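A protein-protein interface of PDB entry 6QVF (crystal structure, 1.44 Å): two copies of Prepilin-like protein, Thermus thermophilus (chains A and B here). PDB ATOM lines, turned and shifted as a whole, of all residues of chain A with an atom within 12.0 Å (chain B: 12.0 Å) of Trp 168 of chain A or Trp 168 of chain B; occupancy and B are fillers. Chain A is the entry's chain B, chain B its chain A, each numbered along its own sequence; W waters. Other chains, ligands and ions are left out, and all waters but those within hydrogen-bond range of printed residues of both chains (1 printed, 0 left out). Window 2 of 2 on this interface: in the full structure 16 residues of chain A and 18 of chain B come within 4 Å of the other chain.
The backbone carbonyl oxygen (O) of Ser 167 of chain B lies within hydrogen-bond range of the backbone NH (N) of Ser 169 of chain A, at 2.7 Å.
N of Ser 169 of chain B lies within hydrogen-bond range of O of Ser 167 of chain A (2.9 Å).
The backbone carbonyl oxygen (O) of Ser 167 of chain B sits close to the backbone carbonyl oxygen (O) of Ser 167 of chain A.
Among the printed residues, pairs that only touch across the chains: Gly 164 of chain A with Pro 171 of chain B (3.4 Å), Gly 166 of chain A with Ser 169 of chain B (3.3 Å), Ser 167 of chain A with Trp 168 of chain B (3.6 Å), Trp 168 of chain A with Ser 167 of chain B (3.6 Å), Trp 168 of chain A with Trp 168 of chain B (3.5 Å), Ser 169 of chain A with Gly 166 of chain B (3.3 Å) and Pro 171 of chain A with Gly 164 of chain B (3.4 Å).
Asn 110 of chain A touches none of the printed residues of chain B.
Of the printed residues of chain B, Gly 164 of chain A touches Pro 171.
Gly 166 of chain A touches one residue of chain B.
Of chain B, only Ser 167 (3.3 Å), Trp 168 (3.6 Å) and Ser 169 (2.9 Å) come within 4 Å of Ser 167 of chain A.
Trp 168 of chain A touches two residues of chain B.
Ser 169 of chain A touches just these residues of chain B: Gly 166 (3.3 Å) and Ser 167 (2.7 Å).
His 170 of chain A touches none of the printed residues of chain B.
Printed residues of chain B within 4 Å of Pro 171 of chain A: Gly 164.
Of the printed residues of chain A, Gly 164 of chain B touches Pro 171 (3.4 Å).
Of chain A, only Ser 167 (3.3 Å), Trp 168 (3.6 Å) and Ser 169 (2.7 Å) come within 4 Å of Ser 167 of chain B.
Of the printed residues of chain A, Trp 168 of chain B touches Ser 167 and Trp 168.
Ser 169 of chain B touches two residues of chain A.
No residue of chain A comes within 4 Å of His 170 of chain B.
Printed residues of chain A within 4 Å of Pro 171 of chain B: Gly 164.
Phe 173 of chain B touches none of the printed residues of chain A.
Printed residues of chain B that touch a printed residue of chain A: Gly 164, Gly 166, Ser 167, Trp 168, Ser 169 and Pro 171.
Hydrophobic or aromatic side chains of chain B that line the printed part of chain A: Trp 168 and Pro 171.
Of the 14 printed residues of chain A, 6 touch a printed residue of chain B.
Among the printed residues, no Asp or Glu carboxylate lies within 4 Å of a Lys or Arg side-chain nitrogen of the other chain.
Gly 164 of chain A touches Pro 171 of chain B, and with the chains exchanged Pro 171 of chain A touches Gly 164 of chain B.
Gly 166 of chain A touches Ser 169 of chain B, and with the chains exchanged Ser 169 of chain A touches Gly 166 of chain B.
Ser 167 of chain A touches Trp 168 of chain B, and with the chains exchanged Trp 168 of chain A touches Ser 167 of chain B.
Trp 168 of chain A touches its own counterpart, Trp 168 of chain B.
Positions printed for both chains: 110, 111, 112, 113, 164, 165, 166, 167, 168, 169, 170, 171, 172 and 173.
Water W1 bridges the side-chain hydroxyl of Ser 167 of chain A (2.8 Å) and the backbone carbonyl oxygen of Ser 167 of chain B (3.0 Å).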
ATOM      1  N   ASN A 110     -20.792  19.381  13.162  1.00  0.00           N
ATOM      2  CA  ASN A 110     -21.132  18.216  13.930  1.00  0.00           C
ATOM      3  C   ASN A 110     -20.894  16.933  13.128  1.00  0.00           C
ATOM      4  O   ASN A 110     -20.579  16.972  11.940  1.00  0.00           O
ATOM      5  CB  ASN A 110     -22.549  18.297  14.456  1.00  0.00           C
ATOM      6  CG  ASN A 110     -23.547  18.406  13.351  1.00  0.00           C
ATOM      7  OD1 ASN A 110     -23.742  17.408  12.629  1.00  0.00           O
ATOM      8  ND2 ASN A 110     -24.187  19.578  13.256  1.00  0.00           N
ATOM      9  N   GLY A 111     -20.966  15.806  13.851  1.00  0.00           N
ATOM     10  CA  GLY A 111     -20.664  14.528  13.288  1.00  0.00           C
ATOM     11  C   GLY A 111     -19.188  14.348  13.029  1.00  0.00           C
ATOM     12  O   GLY A 111     -18.352  15.200  13.338  1.00  0.00           O
ATOM     13  N   ILE A 112     -18.856  13.222  12.408  1.00  0.00           N
ATOM     14  CA  ILE A 112     -17.470  12.864  12.213  1.00  0.00           C
ATOM     15  C   ILE A 112     -16.796  13.885  11.280  1.00  0.00           C
ATOM     16  O   ILE A 112     -15.655  14.320  11.563  1.00  0.00           O
ATOM     17  CB  ILE A 112     -17.369  11.416  11.720  1.00  0.00           C
ATOM     18  CG1 ILE A 112     -15.923  10.968  11.693  1.00  0.00           C
ATOM     19  CG2 ILE A 112     -18.005  11.233  10.368  1.00  0.00           C
ATOM     20  CD1 ILE A 112     -15.386  10.840  13.055  1.00  0.00           C
ATOM     21  N   LEU A 113     -17.526  14.342  10.262  1.00  0.00           N
ATOM     22  CA  LEU A 113     -17.037  15.325   9.290  1.00  0.00           C
ATOM     23  C   LEU A 113     -16.741  16.678   9.976  1.00  0.00           C
ATOM     24  O   LEU A 113     -15.812  17.426   9.606  1.00  0.00           O
ATOM     25  CB  LEU A 113     -18.101  15.528   8.213  1.00  0.00           C
ATOM     26  CG  LEU A 113     -17.717  15.169   6.779  1.00  0.00           C
ATOM     27  CD1 LEU A 113     -18.737  15.735   5.829  1.00  0.00           C
ATOM     28  CD2 LEU A 113     -16.349  15.680   6.412  1.00  0.00           C
ATOM     29  N   GLY A 164     -23.469  14.093  15.618  1.00  0.00           N
ATOM     30  CA  GLY A 164     -24.045  14.291  14.304  1.00  0.00           C
ATOM     31  C   GLY A 164     -25.542  14.618  14.368  1.00  0.00           C
ATOM     32  O   GLY A 164     -26.320  14.018  15.107  1.00  0.00           O
ATOM     33  N   SER A 165     -25.980  15.571  13.540  1.00  0.00           N
ATOM     34  CA  SER A 165     -27.386  16.020  13.586  1.00  0.00           C
ATOM     35  C   SER A 165     -28.257  15.151  12.677  1.00  0.00           C
ATOM     36  O   SER A 165     -29.473  15.000  12.962  1.00  0.00           O
ATOM     37  CB  SER A 165     -27.554  17.497  13.299  1.00  0.00           C
ATOM     38  OG  SER A 165     -26.840  17.834  12.147  1.00  0.00           O
ATOM     39  N   GLY A 166     -27.670  14.599  11.614  1.00  0.00           N
ATOM     40  CA  GLY A 166     -28.431  13.758  10.692  1.00  0.00           C
ATOM     41  C   GLY A 166     -29.127  14.585   9.623  1.00  0.00           C
ATOM     42  O   GLY A 166     -29.678  15.615   9.891  1.00  0.00           O
ATOM     43  N   SER A 167     -29.137  14.058   8.401  1.00  0.00           N
ATOM     44  CA  SER A 167     -29.838  14.670   7.299  1.00  0.00           C
ATOM     45  C   SER A 167     -29.990  13.624   6.193  1.00  0.00           C
ATOM     46  O   SER A 167     -29.041  13.029   5.758  1.00  0.00           O
ATOM     47  CB  SER A 167     -29.048  15.875   6.777  1.00  0.00           C
ATOM     48  OG  SER A 167     -29.656  16.395   5.595  1.00  0.00           O
ATOM     49  N   TRP A 168     -31.213  13.454   5.732  1.00  0.00           N
ATOM     50  CA  TRP A 168     -31.469  12.554   4.664  1.00  0.00           C
ATOM     51  C   TRP A 168     -32.002  13.367   3.497  1.00  0.00           C
ATOM     52  O   TRP A 168     -33.138  13.799   3.520  1.00  0.00           O
ATOM     53  CB  TRP A 168     -32.490  11.508   5.083  1.00  0.00           C
ATOM     54  CG  TRP A 168     -32.602  10.334   4.143  1.00  0.00           C
ATOM     55  CD1 TRP A 168     -31.939  10.112   2.966  1.00  0.00           C
ATOM     56  CD2 TRP A 168     -33.453   9.202   4.345  1.00  0.00           C
ATOM     57  NE1 TRP A 168     -32.365   8.939   2.398  1.00  0.00           N
ATOM     58  CE2 TRP A 168     -33.313   8.370   3.223  1.00  0.00           C
ATOM     59  CE3 TRP A 168     -34.359   8.839   5.352  1.00  0.00           C
ATOM     60  CZ2 TRP A 168     -33.975   7.148   3.143  1.00  0.00           C
ATOM     61  CZ3 TRP A 168     -35.033   7.651   5.253  1.00  0.00           C
ATOM     62  CH2 TRP A 168     -34.864   6.832   4.139  1.00  0.00           C
ATOM     63  N   SER A 169     -31.146  13.568   2.493  1.00  0.00           N
ATOM     64  CA  SER A 169     -31.460  14.351   1.325  1.00  0.00           C
ATOM     65  C   SER A 169     -31.567  13.447   0.110  1.00  0.00           C
ATOM     66  O   SER A 169     -30.699  12.633  -0.114  1.00  0.00           O
ATOM     67  CB  SER A 169     -30.327  15.367   1.104  1.00  0.00           C
ATOM     68  OG  SER A 169     -30.673  16.188   0.053  1.00  0.00           O
ATOM     69  N   HIS A 170     -32.572  13.680  -0.748  1.00  0.00           N
ATOM     70  CA  HIS A 170     -32.714  12.869  -1.967  1.00  0.00           C
ATOM     71  C   HIS A 170     -33.663  13.575  -2.905  1.00  0.00           C
ATOM     72  O   HIS A 170     -34.671  14.117  -2.461  1.00  0.00           O
ATOM     73  CB  HIS A 170     -33.251  11.466  -1.627  1.00  0.00           C
ATOM     74  CG  HIS A 170     -33.018  10.481  -2.712  1.00  0.00           C
ATOM     75  ND1 HIS A 170     -33.717  10.512  -3.891  1.00  0.00           N
ATOM     76  CD2 HIS A 170     -32.183   9.437  -2.775  1.00  0.00           C
ATOM     77  CE1 HIS A 170     -33.276   9.554  -4.671  1.00  0.00           C
ATOM     78  NE2 HIS A 170     -32.347   8.845  -3.977  1.00  0.00           N
ATOM     79  N   PRO A 171     -33.384  13.573  -4.217  1.00  0.00           N
ATOM     80  CA  PRO A 171     -34.293  14.245  -5.142  1.00  0.00           C
ATOM     81  C   PRO A 171     -35.696  13.623  -5.164  1.00  0.00           C
ATOM     82  O   PRO A 171     -36.671  14.280  -5.505  1.00  0.00           O
ATOM     83  CB  PRO A 171     -33.599  14.106  -6.504  1.00  0.00           C
ATOM     84  CG  PRO A 171     -32.454  13.167  -6.336  1.00  0.00           C
ATOM     85  CD  PRO A 171     -32.169  13.040  -4.866  1.00  0.00           C
ATOM     86  N   GLN A 172     -35.804  12.344  -4.793  1.00  0.00           N
ATOM     87  CA  GLN A 172     -37.104  11.684  -4.710  1.00  0.00           C
ATOM     88  C   GLN A 172     -38.020  12.404  -3.714  1.00  0.00           C
ATOM     89  O   GLN A 172     -39.247  12.302  -3.826  1.00  0.00           O
ATOM     90  CB  GLN A 172     -36.912  10.216  -4.310  1.00  0.00           C
ATOM     91  CG  GLN A 172     -38.143   9.358  -4.532  1.00  0.00           C
ATOM     92  CD  GLN A 172     -37.835   7.935  -4.129  1.00  0.00           C
ATOM     93  OE1 GLN A 172     -38.163   7.506  -3.023  1.00  0.00           O
ATOM     94  NE2 GLN A 172     -37.148   7.239  -5.005  1.00  0.00           N
ATOM     95  N   PHE A 173     -37.431  13.130  -2.752  1.00  0.00           N
ATOM     96  CA  PHE A 173     -38.198  13.834  -1.739  1.00  0.00           C
ATOM     97  C   PHE A 173     -38.656  15.225  -2.255  1.00  0.00           C
ATOM     98  O   PHE A 173     -39.402  15.863  -1.431  1.00  0.00           O
ATOM     99  CB  PHE A 173     -37.408  13.983  -0.425  1.00  0.00           C
ATOM    100  CG  PHE A 173     -36.767  12.729   0.134  1.00  0.00           C
ATOM    101  CD1 PHE A 173     -37.228  11.471  -0.209  1.00  0.00           C
ATOM    102  CD2 PHE A 173     -35.699  12.783   1.017  1.00  0.00           C
ATOM    103  CE1 PHE A 173     -36.651  10.325   0.301  1.00  0.00           C
ATOM    104  CE2 PHE A 173     -35.111  11.627   1.526  1.00  0.00           C
ATOM    105  CZ  PHE A 173     -35.565  10.392   1.136  1.00  0.00           C
ATOM    106  N   ASN B 110     -26.674  21.895  -5.993  1.00  0.00           N
ATOM    107  CA  ASN B 110     -27.655  21.028  -6.624  1.00  0.00           C
ATOM    108  C   ASN B 110     -28.858  20.825  -5.719  1.00  0.00           C
ATOM    109  O   ASN B 110     -28.845  21.227  -4.561  1.00  0.00           O
ATOM    110  CB  ASN B 110     -27.042  19.720  -7.076  1.00  0.00           C
ATOM    111  CG  ASN B 110     -26.442  18.954  -5.951  1.00  0.00           C
ATOM    112  OD1 ASN B 110     -27.194  18.480  -5.070  1.00  0.00           O
ATOM    113  ND2 ASN B 110     -25.116  18.839  -5.986  1.00  0.00           N
ATOM    114  N   GLY B 111     -29.896  20.212  -6.308  1.00  0.00           N
ATOM    115  CA  GLY B 111     -31.152  20.030  -5.610  1.00  0.00           C
ATOM    116  C   GLY B 111     -31.939  21.325  -5.489  1.00  0.00           C
ATOM    117  O   GLY B 111     -31.525  22.383  -5.950  1.00  0.00           O
ATOM    118  N   ILE B 112     -33.118  21.256  -4.862  1.00  0.00           N
ATOM    119  CA  ILE B 112     -33.986  22.439  -4.850  1.00  0.00           C
ATOM    120  C   ILE B 112     -33.292  23.578  -4.096  1.00  0.00           C
ATOM    121  O   ILE B 112     -33.371  24.709  -4.549  1.00  0.00           O
ATOM    122  CB  ILE B 112     -35.367  22.138  -4.252  1.00  0.00           C
ATOM    123  CG1 ILE B 112     -35.225  21.455  -2.894  1.00  0.00           C
ATOM    124  CG2 ILE B 112     -36.183  21.325  -5.233  1.00  0.00           C
ATOM    125  CD1 ILE B 112     -36.532  20.959  -2.338  1.00  0.00           C
ATOM    126  N   LEU B 113     -32.614  23.237  -2.996  1.00  0.00           N
ATOM    127  CA  LEU B 113     -31.918  24.153  -2.142  1.00  0.00           C
ATOM    128  C   LEU B 113     -30.776  24.854  -2.888  1.00  0.00           C
ATOM    129  O   LEU B 113     -30.434  25.994  -2.568  1.00  0.00           O
ATOM    130  CB  LEU B 113     -31.319  23.383  -0.967  1.00  0.00           C
ATOM    131  CG  LEU B 113     -31.228  24.227   0.299  1.00  0.00           C
ATOM    132  CD1 LEU B 113     -32.608  24.704   0.705  1.00  0.00           C
ATOM    133  CD2 LEU B 113     -30.608  23.466   1.434  1.00  0.00           C
ATOM    134  N   GLY B 164     -30.525  17.087  -7.706  1.00  0.00           N
ATOM    135  CA  GLY B 164     -30.021  16.740  -6.365  1.00  0.00           C
ATOM    136  C   GLY B 164     -29.106  15.520  -6.384  1.00  0.00           C
ATOM    137  O   GLY B 164     -29.395  14.509  -7.021  1.00  0.00           O
ATOM    138  N   SER B 165     -27.997  15.585  -5.647  1.00  0.00           N
ATOM    139  CA  SER B 165     -27.000  14.494  -5.677  1.00  0.00           C
ATOM    140  C   SER B 165     -27.340  13.410  -4.643  1.00  0.00           C
ATOM    141  O   SER B 165     -26.929  12.243  -4.821  1.00  0.00           O
ATOM    142  CB  SER B 165     -25.579  15.041  -5.478  1.00  0.00           C
ATOM    143  OG  SER B 165     -25.559  15.822  -4.315  1.00  0.00           O
ATOM    144  N   GLY B 166     -28.065  13.782  -3.581  1.00  0.00           N
ATOM    145  CA  GLY B 166     -28.450  12.828  -2.572  1.00  0.00           C
ATOM    146  C   GLY B 166     -27.384  12.671  -1.495  1.00  0.00           C
ATOM    147  O   GLY B 166     -26.225  12.543  -1.768  1.00  0.00           O
ATOM    148  N   SER B 167     -27.804  12.601  -0.242  1.00  0.00           N
ATOM    149  CA  SER B 167     -26.866  12.338   0.852  1.00  0.00           C
ATOM    150  C   SER B 167     -27.673  11.860   2.052  1.00  0.00           C
ATOM    151  O   SER B 167     -28.620  12.512   2.479  1.00  0.00           O
ATOM    152  CB  SER B 167     -26.105  13.597   1.220  1.00  0.00           C
ATOM    153  OG  SER B 167     -25.188  13.319   2.279  1.00  0.00           O
ATOM    154  N   TRP B 168     -27.230  10.761   2.644  1.00  0.00           N
ATOM    155  CA  TRP B 168     -27.889  10.248   3.824  1.00  0.00           C
ATOM    156  C   TRP B 168     -26.862  10.171   4.957  1.00  0.00           C
ATOM    157  O   TRP B 168     -26.028   9.270   4.977  1.00  0.00           O
ATOM    158  CB  TRP B 168     -28.500   8.866   3.533  1.00  0.00           C
ATOM    159  CG  TRP B 168     -29.420   8.353   4.596  1.00  0.00           C
ATOM    160  CD1 TRP B 168     -29.789   8.978   5.746  1.00  0.00           C
ATOM    161  CD2 TRP B 168     -30.125   7.105   4.566  1.00  0.00           C
ATOM    162  NE1 TRP B 168     -30.645   8.182   6.458  1.00  0.00           N
ATOM    163  CE2 TRP B 168     -30.892   7.032   5.733  1.00  0.00           C
ATOM    164  CE3 TRP B 168     -30.172   6.039   3.669  1.00  0.00           C
ATOM    165  CZ2 TRP B 168     -31.657   5.912   6.038  1.00  0.00           C
ATOM    166  CZ3 TRP B 168     -30.919   4.921   3.971  1.00  0.00           C
ATOM    167  CH2 TRP B 168     -31.692   4.879   5.129  1.00  0.00           C
ATOM    168  N   SER B 169     -26.906  11.133   5.872  1.00  0.00           N
ATOM    169  CA  SER B 169     -25.963  11.086   6.987  1.00  0.00           C
ATOM    170  C   SER B 169     -26.738  10.873   8.283  1.00  0.00           C
ATOM    171  O   SER B 169     -27.829  11.357   8.474  1.00  0.00           O
ATOM    172  CB  SER B 169     -25.095  12.291   7.083  1.00  0.00           C
ATOM    173  OG  SER B 169     -25.866  13.407   7.308  1.00  0.00           O
ATOM    174  N   HIS B 170     -26.100  10.164   9.194  1.00  0.00           N
ATOM    175  CA  HIS B 170     -26.698   9.844  10.464  1.00  0.00           C
ATOM    176  C   HIS B 170     -25.595   9.341  11.371  1.00  0.00           C
ATOM    177  O   HIS B 170     -24.705   8.614  10.942  1.00  0.00           O
ATOM    178  CB  HIS B 170     -27.764   8.758  10.276  1.00  0.00           C
ATOM    179  CG  HIS B 170     -28.702   8.669  11.423  1.00  0.00           C
ATOM    180  ND1 HIS B 170     -28.318   8.122  12.638  1.00  0.00           N
ATOM    181  CD2 HIS B 170     -29.995   8.968  11.528  1.00  0.00           C
ATOM    182  CE1 HIS B 170     -29.346   8.188  13.469  1.00  0.00           C
ATOM    183  NE2 HIS B 170     -30.368   8.720  12.818  1.00  0.00           N
ATOM    184  N   PRO B 171     -25.614   9.733  12.651  1.00  0.00           N
ATOM    185  CA  PRO B 171     -24.596   9.266  13.585  1.00  0.00           C
ATOM    186  C   PRO B 171     -24.563   7.756  13.744  1.00  0.00           C
ATOM    187  O   PRO B 171     -23.489   7.162  14.047  1.00  0.00           O
ATOM    188  CB  PRO B 171     -24.955   9.912  14.921  1.00  0.00           C
ATOM    189  CG  PRO B 171     -26.219  10.652  14.730  1.00  0.00           C
ATOM    190  CD  PRO B 171     -26.559  10.663  13.254  1.00  0.00           C
ATOM    191  N   GLN B 172     -25.696   7.111  13.470  1.00  0.00           N
ATOM    192  CA  GLN B 172     -25.747   5.662  13.563  1.00  0.00           C
ATOM    193  C   GLN B 172     -24.805   4.988  12.540  1.00  0.00           C
ATOM    194  O   GLN B 172     -24.345   3.833  12.748  1.00  0.00           O
ATOM    195  CB  GLN B 172     -27.195   5.229  13.384  1.00  0.00           C
ATOM    196  CG  GLN B 172     -27.461   3.779  13.714  1.00  0.00           C
ATOM    197  CD  GLN B 172     -28.895   3.436  13.413  1.00  0.00           C
ATOM    198  OE1 GLN B 172     -29.201   2.822  12.391  1.00  0.00           O
ATOM    199  NE2 GLN B 172     -29.784   3.828  14.299  1.00  0.00           N
ATOM    200  N   PHE B 173     -24.470   5.708  11.463  1.00  0.00           N
ATOM    201  CA  PHE B 173     -23.597   5.232  10.405  1.00  0.00           C
ATOM    202  C   PHE B 173     -22.122   5.418  10.804  1.00  0.00           C
ATOM    203  O   PHE B 173     -21.300   4.956   9.990  1.00  0.00           O
ATOM    204  CB  PHE B 173     -23.892   5.916   9.056  1.00  0.00           C
ATOM    205  CG  PHE B 173     -25.320   5.901   8.590  1.00  0.00           C
ATOM    206  CD1 PHE B 173     -26.225   4.978   9.089  1.00  0.00           C
ATOM    207  CD2 PHE B 173     -25.776   6.820   7.650  1.00  0.00           C
ATOM    208  CE1 PHE B 173     -27.551   5.034   8.708  1.00  0.00           C
ATOM    209  CE2 PHE B 173     -27.102   6.843   7.242  1.00  0.00           C
ATOM    210  CZ  PHE B 173     -27.984   5.930   7.761  1.00  0.00           C
HETATM  211  O   HOH W   1     -27.839  15.120   3.828  1.00  0.00           O
